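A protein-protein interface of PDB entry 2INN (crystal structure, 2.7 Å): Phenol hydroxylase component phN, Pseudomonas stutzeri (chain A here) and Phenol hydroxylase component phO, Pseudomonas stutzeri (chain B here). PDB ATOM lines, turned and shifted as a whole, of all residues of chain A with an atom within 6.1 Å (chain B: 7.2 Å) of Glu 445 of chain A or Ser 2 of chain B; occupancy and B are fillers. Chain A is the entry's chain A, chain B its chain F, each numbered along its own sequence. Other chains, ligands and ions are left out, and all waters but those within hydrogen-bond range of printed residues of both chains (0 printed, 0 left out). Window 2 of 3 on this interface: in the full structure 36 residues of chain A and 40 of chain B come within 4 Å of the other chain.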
ATOM      1  N   HIS A 424      10.415  10.510  -3.640  1.00  0.00           N
ATOM      2  CA  HIS A 424      10.117   9.862  -4.843  1.00  0.00           C
ATOM      3  C   HIS A 424       8.856  10.459  -5.429  1.00  0.00           C
ATOM      4  O   HIS A 424       7.838  10.411  -4.758  1.00  0.00           O
ATOM      5  CB  HIS A 424       9.995   8.364  -4.601  1.00  0.00           C
ATOM      6  CG  HIS A 424       9.384   7.627  -5.749  1.00  0.00           C
ATOM      7  ND1 HIS A 424       8.013   7.414  -5.855  1.00  0.00           N
ATOM      8  CD2 HIS A 424       9.939   7.103  -6.868  1.00  0.00           C
ATOM      9  CE1 HIS A 424       7.755   6.781  -6.991  1.00  0.00           C
ATOM     10  NE2 HIS A 424       8.899   6.619  -7.638  1.00  0.00           N
ATOM     11  N   PHE A 440      11.972  -0.571  -1.007  1.00  0.00           N
ATOM     12  CA  PHE A 440      11.165   0.524  -1.522  1.00  0.00           C
ATOM     13  C   PHE A 440      11.602   0.994  -2.941  1.00  0.00           C
ATOM     14  O   PHE A 440      10.792   1.075  -3.883  1.00  0.00           O
ATOM     15  CB  PHE A 440      11.210   1.783  -0.602  1.00  0.00           C
ATOM     16  CG  PHE A 440      10.206   2.820  -1.024  1.00  0.00           C
ATOM     17  CD1 PHE A 440       8.821   2.631  -0.730  1.00  0.00           C
ATOM     18  CD2 PHE A 440      10.579   3.867  -1.840  1.00  0.00           C
ATOM     19  CE1 PHE A 440       7.797   3.505  -1.211  1.00  0.00           C
ATOM     20  CE2 PHE A 440       9.618   4.739  -2.299  1.00  0.00           C
ATOM     21  CZ  PHE A 440       8.191   4.555  -1.943  1.00  0.00           C
ATOM     22  N   LYS A 441      12.903   1.343  -2.989  1.00  0.00           N
ATOM     23  CA  LYS A 441      13.557   1.866  -4.135  1.00  0.00           C
ATOM     24  C   LYS A 441      13.397   0.829  -5.204  1.00  0.00           C
ATOM     25  O   LYS A 441      13.199   1.224  -6.368  1.00  0.00           O
ATOM     26  CB  LYS A 441      15.039   2.128  -3.908  1.00  0.00           C
ATOM     27  CG  LYS A 441      15.314   3.395  -3.196  1.00  0.00           C
ATOM     28  CD  LYS A 441      16.604   3.386  -2.290  1.00  0.00           C
ATOM     29  CE  LYS A 441      17.749   2.672  -2.967  1.00  0.00           C
ATOM     30  NZ  LYS A 441      18.796   2.410  -1.933  1.00  0.00           N
ATOM     31  N   HIS A 442      13.446  -0.468  -4.863  1.00  0.00           N
ATOM     32  CA  HIS A 442      13.280  -1.441  -5.952  1.00  0.00           C
ATOM     33  C   HIS A 442      11.843  -1.442  -6.565  1.00  0.00           C
ATOM     34  O   HIS A 442      11.765  -1.681  -7.743  1.00  0.00           O
ATOM     35  CB  HIS A 442      13.914  -2.876  -5.754  1.00  0.00           C
ATOM     36  CG  HIS A 442      13.842  -3.714  -7.016  1.00  0.00           C
ATOM     37  ND1 HIS A 442      12.772  -4.558  -7.315  1.00  0.00           N
ATOM     38  CD2 HIS A 442      14.658  -3.764  -8.111  1.00  0.00           C
ATOM     39  CE1 HIS A 442      12.942  -5.114  -8.511  1.00  0.00           C
ATOM     40  NE2 HIS A 442      14.080  -4.650  -9.015  1.00  0.00           N
ATOM     41  N   GLU A 443      10.757  -1.193  -5.805  1.00  0.00           N
ATOM     42  CA  GLU A 443       9.350  -1.204  -6.314  1.00  0.00           C
ATOM     43  C   GLU A 443       8.539  -0.025  -5.775  1.00  0.00           C
ATOM     44  O   GLU A 443       7.440  -0.137  -5.224  1.00  0.00           O
ATOM     45  CB  GLU A 443       8.591  -2.448  -5.956  1.00  0.00           C
ATOM     46  CG  GLU A 443       9.376  -3.651  -6.111  1.00  0.00           C
ATOM     47  CD  GLU A 443       8.534  -4.913  -5.977  1.00  0.00           C
ATOM     48  OE1 GLU A 443       7.853  -5.282  -6.992  1.00  0.00           O
ATOM     49  OE2 GLU A 443       8.597  -5.553  -4.869  1.00  0.00           O
ATOM     50  N   PRO A 444       9.036   1.155  -6.002  1.00  0.00           N
ATOM     51  CA  PRO A 444       8.357   2.250  -5.347  1.00  0.00           C
ATOM     52  C   PRO A 444       6.905   2.383  -5.749  1.00  0.00           C
ATOM     53  O   PRO A 444       6.150   2.961  -5.059  1.00  0.00           O
ATOM     54  CB  PRO A 444       9.155   3.432  -5.825  1.00  0.00           C
ATOM     55  CG  PRO A 444       9.604   2.909  -7.290  1.00  0.00           C
ATOM     56  CD  PRO A 444      10.118   1.593  -6.888  1.00  0.00           C
ATOM     57  N   GLU A 445       6.489   1.849  -6.857  1.00  0.00           N
ATOM     58  CA  GLU A 445       5.114   2.061  -7.276  1.00  0.00           C
ATOM     59  C   GLU A 445       4.115   1.171  -6.550  1.00  0.00           C
ATOM     60  O   GLU A 445       2.905   1.433  -6.508  1.00  0.00           O
ATOM     61  CB  GLU A 445       5.046   1.982  -8.794  1.00  0.00           C
ATOM     62  CG  GLU A 445       6.457   2.532  -9.327  1.00  0.00           C
ATOM     63  CD  GLU A 445       7.415   1.466 -10.051  1.00  0.00           C
ATOM     64  OE1 GLU A 445       8.083   0.520  -9.491  1.00  0.00           O
ATOM     65  OE2 GLU A 445       7.512   1.666 -11.272  1.00  0.00           O
ATOM     66  N   LYS A 446       4.652   0.130  -5.906  1.00  0.00           N
ATOM     67  CA  LYS A 446       3.845  -0.793  -5.122  1.00  0.00           C
ATOM     68  C   LYS A 446       3.529  -0.047  -3.766  1.00  0.00           C
ATOM     69  O   LYS A 446       2.376   0.266  -3.425  1.00  0.00           O
ATOM     70  CB  LYS A 446       4.656  -2.095  -4.962  1.00  0.00           C
ATOM     71  CG  LYS A 446       3.887  -3.167  -4.316  1.00  0.00           C
ATOM     72  CD  LYS A 446       4.464  -4.521  -4.524  1.00  0.00           C
ATOM     73  CE  LYS A 446       3.423  -5.634  -4.246  1.00  0.00           C
ATOM     74  NZ  LYS A 446       4.197  -6.898  -4.189  1.00  0.00           N
ATOM     75  N   TYR A 447       4.587   0.281  -3.053  1.00  0.00           N
ATOM     76  CA  TYR A 447       4.516   0.687  -1.668  1.00  0.00           C
ATOM     77  C   TYR A 447       3.799   2.083  -1.304  1.00  0.00           C
ATOM     78  O   TYR A 447       3.164   2.287  -0.164  1.00  0.00           O
ATOM     79  CB  TYR A 447       5.967   0.595  -1.169  1.00  0.00           C
ATOM     80  CG  TYR A 447       6.443  -0.823  -1.192  1.00  0.00           C
ATOM     81  CD1 TYR A 447       5.892  -1.760  -0.309  1.00  0.00           C
ATOM     82  CD2 TYR A 447       7.370  -1.241  -2.093  1.00  0.00           C
ATOM     83  CE1 TYR A 447       6.283  -3.100  -0.300  1.00  0.00           C
ATOM     84  CE2 TYR A 447       7.781  -2.549  -2.117  1.00  0.00           C
ATOM     85  CZ  TYR A 447       7.229  -3.506  -1.209  1.00  0.00           C
ATOM     86  OH  TYR A 447       7.608  -4.852  -1.219  1.00  0.00           O
ATOM     87  N   ILE A 448       3.886   3.025  -2.266  1.00  0.00           N
ATOM     88  CA  ILE A 448       3.170   4.247  -2.135  1.00  0.00           C
ATOM     89  C   ILE A 448       1.694   4.032  -2.010  1.00  0.00           C
ATOM     90  O   ILE A 448       1.045   4.952  -1.543  1.00  0.00           O
ATOM     91  CB  ILE A 448       3.498   5.204  -3.254  1.00  0.00           C
ATOM     92  CG1 ILE A 448       2.992   4.706  -4.598  1.00  0.00           C
ATOM     93  CG2 ILE A 448       5.034   5.442  -3.377  1.00  0.00           C
ATOM     94  CD1 ILE A 448       3.232   5.715  -5.625  1.00  0.00           C
ATOM     95  N   GLN A 449       1.173   2.851  -2.370  1.00  0.00           N
ATOM     96  CA  GLN A 449      -0.221   2.409  -2.192  1.00  0.00           C
ATOM     97  C   GLN A 449      -0.596   1.925  -0.771  1.00  0.00           C
ATOM     98  O   GLN A 449      -1.803   1.732  -0.446  1.00  0.00           O
ATOM     99  CB  GLN A 449      -0.448   1.189  -3.085  1.00  0.00           C
ATOM    100  CG  GLN A 449      -0.722   1.494  -4.514  1.00  0.00           C
ATOM    101  CD  GLN A 449      -0.722   0.271  -5.368  1.00  0.00           C
ATOM    102  OE1 GLN A 449      -1.745  -0.377  -5.529  1.00  0.00           O
ATOM    103  NE2 GLN A 449       0.415  -0.036  -5.951  1.00  0.00           N
ATOM    104  N   SER B   2      12.400  -2.189  -9.955  1.00  0.00           N
ATOM    105  CA  SER B   2      11.194  -1.427 -10.444  1.00  0.00           C
ATOM    106  C   SER B   2      10.053  -2.417 -10.719  1.00  0.00           C
ATOM    107  O   SER B   2      10.321  -3.578 -11.049  1.00  0.00           O
ATOM    108  CB  SER B   2      11.603  -0.591 -11.646  1.00  0.00           C
ATOM    109  OG  SER B   2      10.576  -0.655 -12.600  1.00  0.00           O
ATOM    110  N   VAL B   3       8.802  -2.029 -10.539  1.00  0.00           N
ATOM    111  CA  VAL B   3       7.737  -3.078 -10.408  1.00  0.00           C
ATOM    112  C   VAL B   3       7.498  -3.861 -11.712  1.00  0.00           C
ATOM    113  O   VAL B   3       7.761  -3.290 -12.750  1.00  0.00           O
ATOM    114  CB  VAL B   3       6.434  -2.486  -9.997  1.00  0.00           C
ATOM    115  CG1 VAL B   3       5.391  -2.941 -10.906  1.00  0.00           C
ATOM    116  CG2 VAL B   3       6.093  -2.959  -8.776  1.00  0.00           C
ATOM    117  N   ASN B   4       7.035  -5.140 -11.664  1.00  0.00           N
ATOM    118  CA  ASN B   4       6.796  -5.930 -12.907  1.00  0.00           C
ATOM    119  C   ASN B   4       5.431  -6.319 -12.909  1.00  0.00           C
ATOM    120  O   ASN B   4       4.997  -6.786 -11.956  1.00  0.00           O
ATOM    121  CB  ASN B   4       7.662  -7.173 -12.970  1.00  0.00           C
ATOM    122  CG  ASN B   4       9.127  -6.819 -12.813  1.00  0.00           C
ATOM    123  OD1 ASN B   4       9.821  -6.584 -13.816  1.00  0.00           O
ATOM    124  ND2 ASN B   4       9.576  -6.609 -11.515  1.00  0.00           N
ATOM    125  N   ALA B   5       4.692  -6.073 -13.946  1.00  0.00           N
ATOM    126  CA  ALA B   5       3.273  -6.377 -13.875  1.00  0.00           C
ATOM    127  C   ALA B   5       2.753  -6.537 -15.260  1.00  0.00           C
ATOM    128  O   ALA B   5       3.422  -6.124 -16.254  1.00  0.00           O
ATOM    129  CB  ALA B   5       2.486  -5.261 -13.167  1.00  0.00           C
ATOM    130  N   TYR B   9       1.841  -0.158 -14.310  1.00  0.00           N
ATOM    131  CA  TYR B   9       1.446  -0.240 -12.915  1.00  0.00           C
ATOM    132  C   TYR B   9       1.729   1.113 -12.257  1.00  0.00           C
ATOM    133  O   TYR B   9       2.809   1.326 -11.668  1.00  0.00           O
ATOM    134  CB  TYR B   9       2.058  -1.520 -12.236  1.00  0.00           C
ATOM    135  CG  TYR B   9       1.549  -1.968 -10.840  1.00  0.00           C
ATOM    136  CD1 TYR B   9       0.456  -2.842 -10.694  1.00  0.00           C
ATOM    137  CD2 TYR B   9       2.230  -1.546  -9.648  1.00  0.00           C
ATOM    138  CE1 TYR B   9       0.020  -3.242  -9.396  1.00  0.00           C
ATOM    139  CE2 TYR B   9       1.796  -1.928  -8.355  1.00  0.00           C
ATOM    140  CZ  TYR B   9       0.698  -2.759  -8.248  1.00  0.00           C
ATOM    141  OH  TYR B   9       0.303  -3.095  -6.981  1.00  0.00           O
ATOM    142  N   LYS B  10       0.750   2.030 -12.404  1.00  0.00           N
ATOM    143  CA  LYS B  10       0.737   3.416 -11.754  1.00  0.00           C
ATOM    144  C   LYS B  10      -0.470   3.765 -10.858  1.00  0.00           C
ATOM    145  O   LYS B  10      -1.664   3.485 -11.184  1.00  0.00           O
ATOM    146  CB  LYS B  10       0.927   4.582 -12.750  1.00  0.00           C
ATOM    147  CG  LYS B  10       2.374   4.849 -13.113  1.00  0.00           C
ATOM    148  CD  LYS B  10       2.578   4.430 -14.636  1.00  0.00           C
ATOM    149  CE  LYS B  10       4.059   4.255 -15.060  1.00  0.00           C
ATOM    150  NZ  LYS B  10       4.612   3.014 -14.386  1.00  0.00           N
ATOM    151  N   PHE B  11      -0.167   4.402  -9.731  1.00  0.00           N
ATOM    152  CA  PHE B  11      -1.235   4.725  -8.798  1.00  0.00           C
ATOM    153  C   PHE B  11      -0.851   5.960  -8.060  1.00  0.00           C
ATOM    154  O   PHE B  11       0.335   6.259  -7.907  1.00  0.00           O
ATOM    155  CB  PHE B  11      -1.531   3.546  -7.835  1.00  0.00           C
ATOM    156  CG  PHE B  11      -2.012   2.277  -8.539  1.00  0.00           C
ATOM    157  CD1 PHE B  11      -3.394   2.084  -8.845  1.00  0.00           C
ATOM    158  CD2 PHE B  11      -1.110   1.306  -8.945  1.00  0.00           C
ATOM    159  CE1 PHE B  11      -3.875   0.891  -9.509  1.00  0.00           C
ATOM    160  CE2 PHE B  11      -1.595   0.143  -9.656  1.00  0.00           C
ATOM    161  CZ  PHE B  11      -2.978  -0.067  -9.916  1.00  0.00           C
ATOM    162  N   GLU B  12      -1.888   6.694  -7.666  1.00  0.00           N
ATOM    163  CA  GLU B  12      -1.762   7.860  -6.830  1.00  0.00           C
ATOM    164  C   GLU B  12      -1.333   7.383  -5.448  1.00  0.00           C
ATOM    165  O   GLU B  12      -1.896   6.416  -4.988  1.00  0.00           O
ATOM    166  CB  GLU B  12      -3.145   8.525  -6.777  1.00  0.00           C
ATOM    167  CG  GLU B  12      -3.588   9.178  -8.149  1.00  0.00           C
ATOM    168  CD  GLU B  12      -2.539  10.221  -8.763  1.00  0.00           C
ATOM    169  OE1 GLU B  12      -2.698  10.626  -9.961  1.00  0.00           O
ATOM    170  OE2 GLU B  12      -1.550  10.621  -8.067  1.00  0.00           O
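Hydrophobic or aromatic side chains of chain B within 4 Å of the printed part of chain A: Val 3, Tyr 9 and Phe 11.
Of the 11 printed residues of chain A, 6 touch a printed residue of chain B.
Hydrophobic or aromatic side chains of chain A that line the printed part of chain B: His 442 and Ile 448.
Among the printed residues, 9 pairs touch across the chains.
O of Glu 445 of chain A sits at hydrogen-bond distance from NE2 of Gln 449 of chain A, at 2.9 Å.
The side-chain amide nitrogen of Gln 449 of chain A sits close to the backbone carbonyl oxygen of Lys 446 of chain A (3.2 Å).
ND2 of Asn 4 of chain B lies within hydrogen-bond range of O of Ser 2 of chain B (3.2 Å).
A ring nitrogen (NE2) of His 442 of chain A sits at hydrogen-bond distance from the backbone NH of Ser 2 of chain B.
The backbone NH of Val 3 of chain B sits at hydrogen-bond distance from the side-chain carboxylate of Glu 445 of chain A (2.8 Å).
NE2 of Gln 449 of chain A lies within hydrogen-bond range of OH of Tyr 9 of chain B, at 3.2 Å.
Among the printed residues, merely in contact across the chains: Glu 443 of chain A with Val 3 of chain B, Gln 449 of chain A with Phe 11 of chain B, Glu 445 of chain A with Tyr 9 of chain B, Ile 448 of chain A with Phe 11 of chain B, Glu 445 of chain A with Ser 2 of chain B and Lys 446 of chain A with Tyr 9 of chain B.
Glu 445 of chain A touches three residues of chain B.
Ser 2 of chain B touches just these residues of chain A: His 442 (2.4 Å) and Glu 445 (3.7 Å).
Of the printed residues of chain A, Tyr 9 of chain B touches Glu 445 (3.7 Å), Lys 446 (3.99 Å) and Gln 449 (3.2 Å).
Of the printed residues of chain B, Lys 446 of chain A touches Tyr 9 (3.99 Å).
Pro 444 of chain A touches none of the printed residues of chain B.
The nearest residue of chain B that does not touch Glu 445 of chain A is Lys 10 of chain B (4.5 Å).
The nearest residue of chain A that does not touch Ser 2 of chain B is Glu 443 of chain A (4.5 Å).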
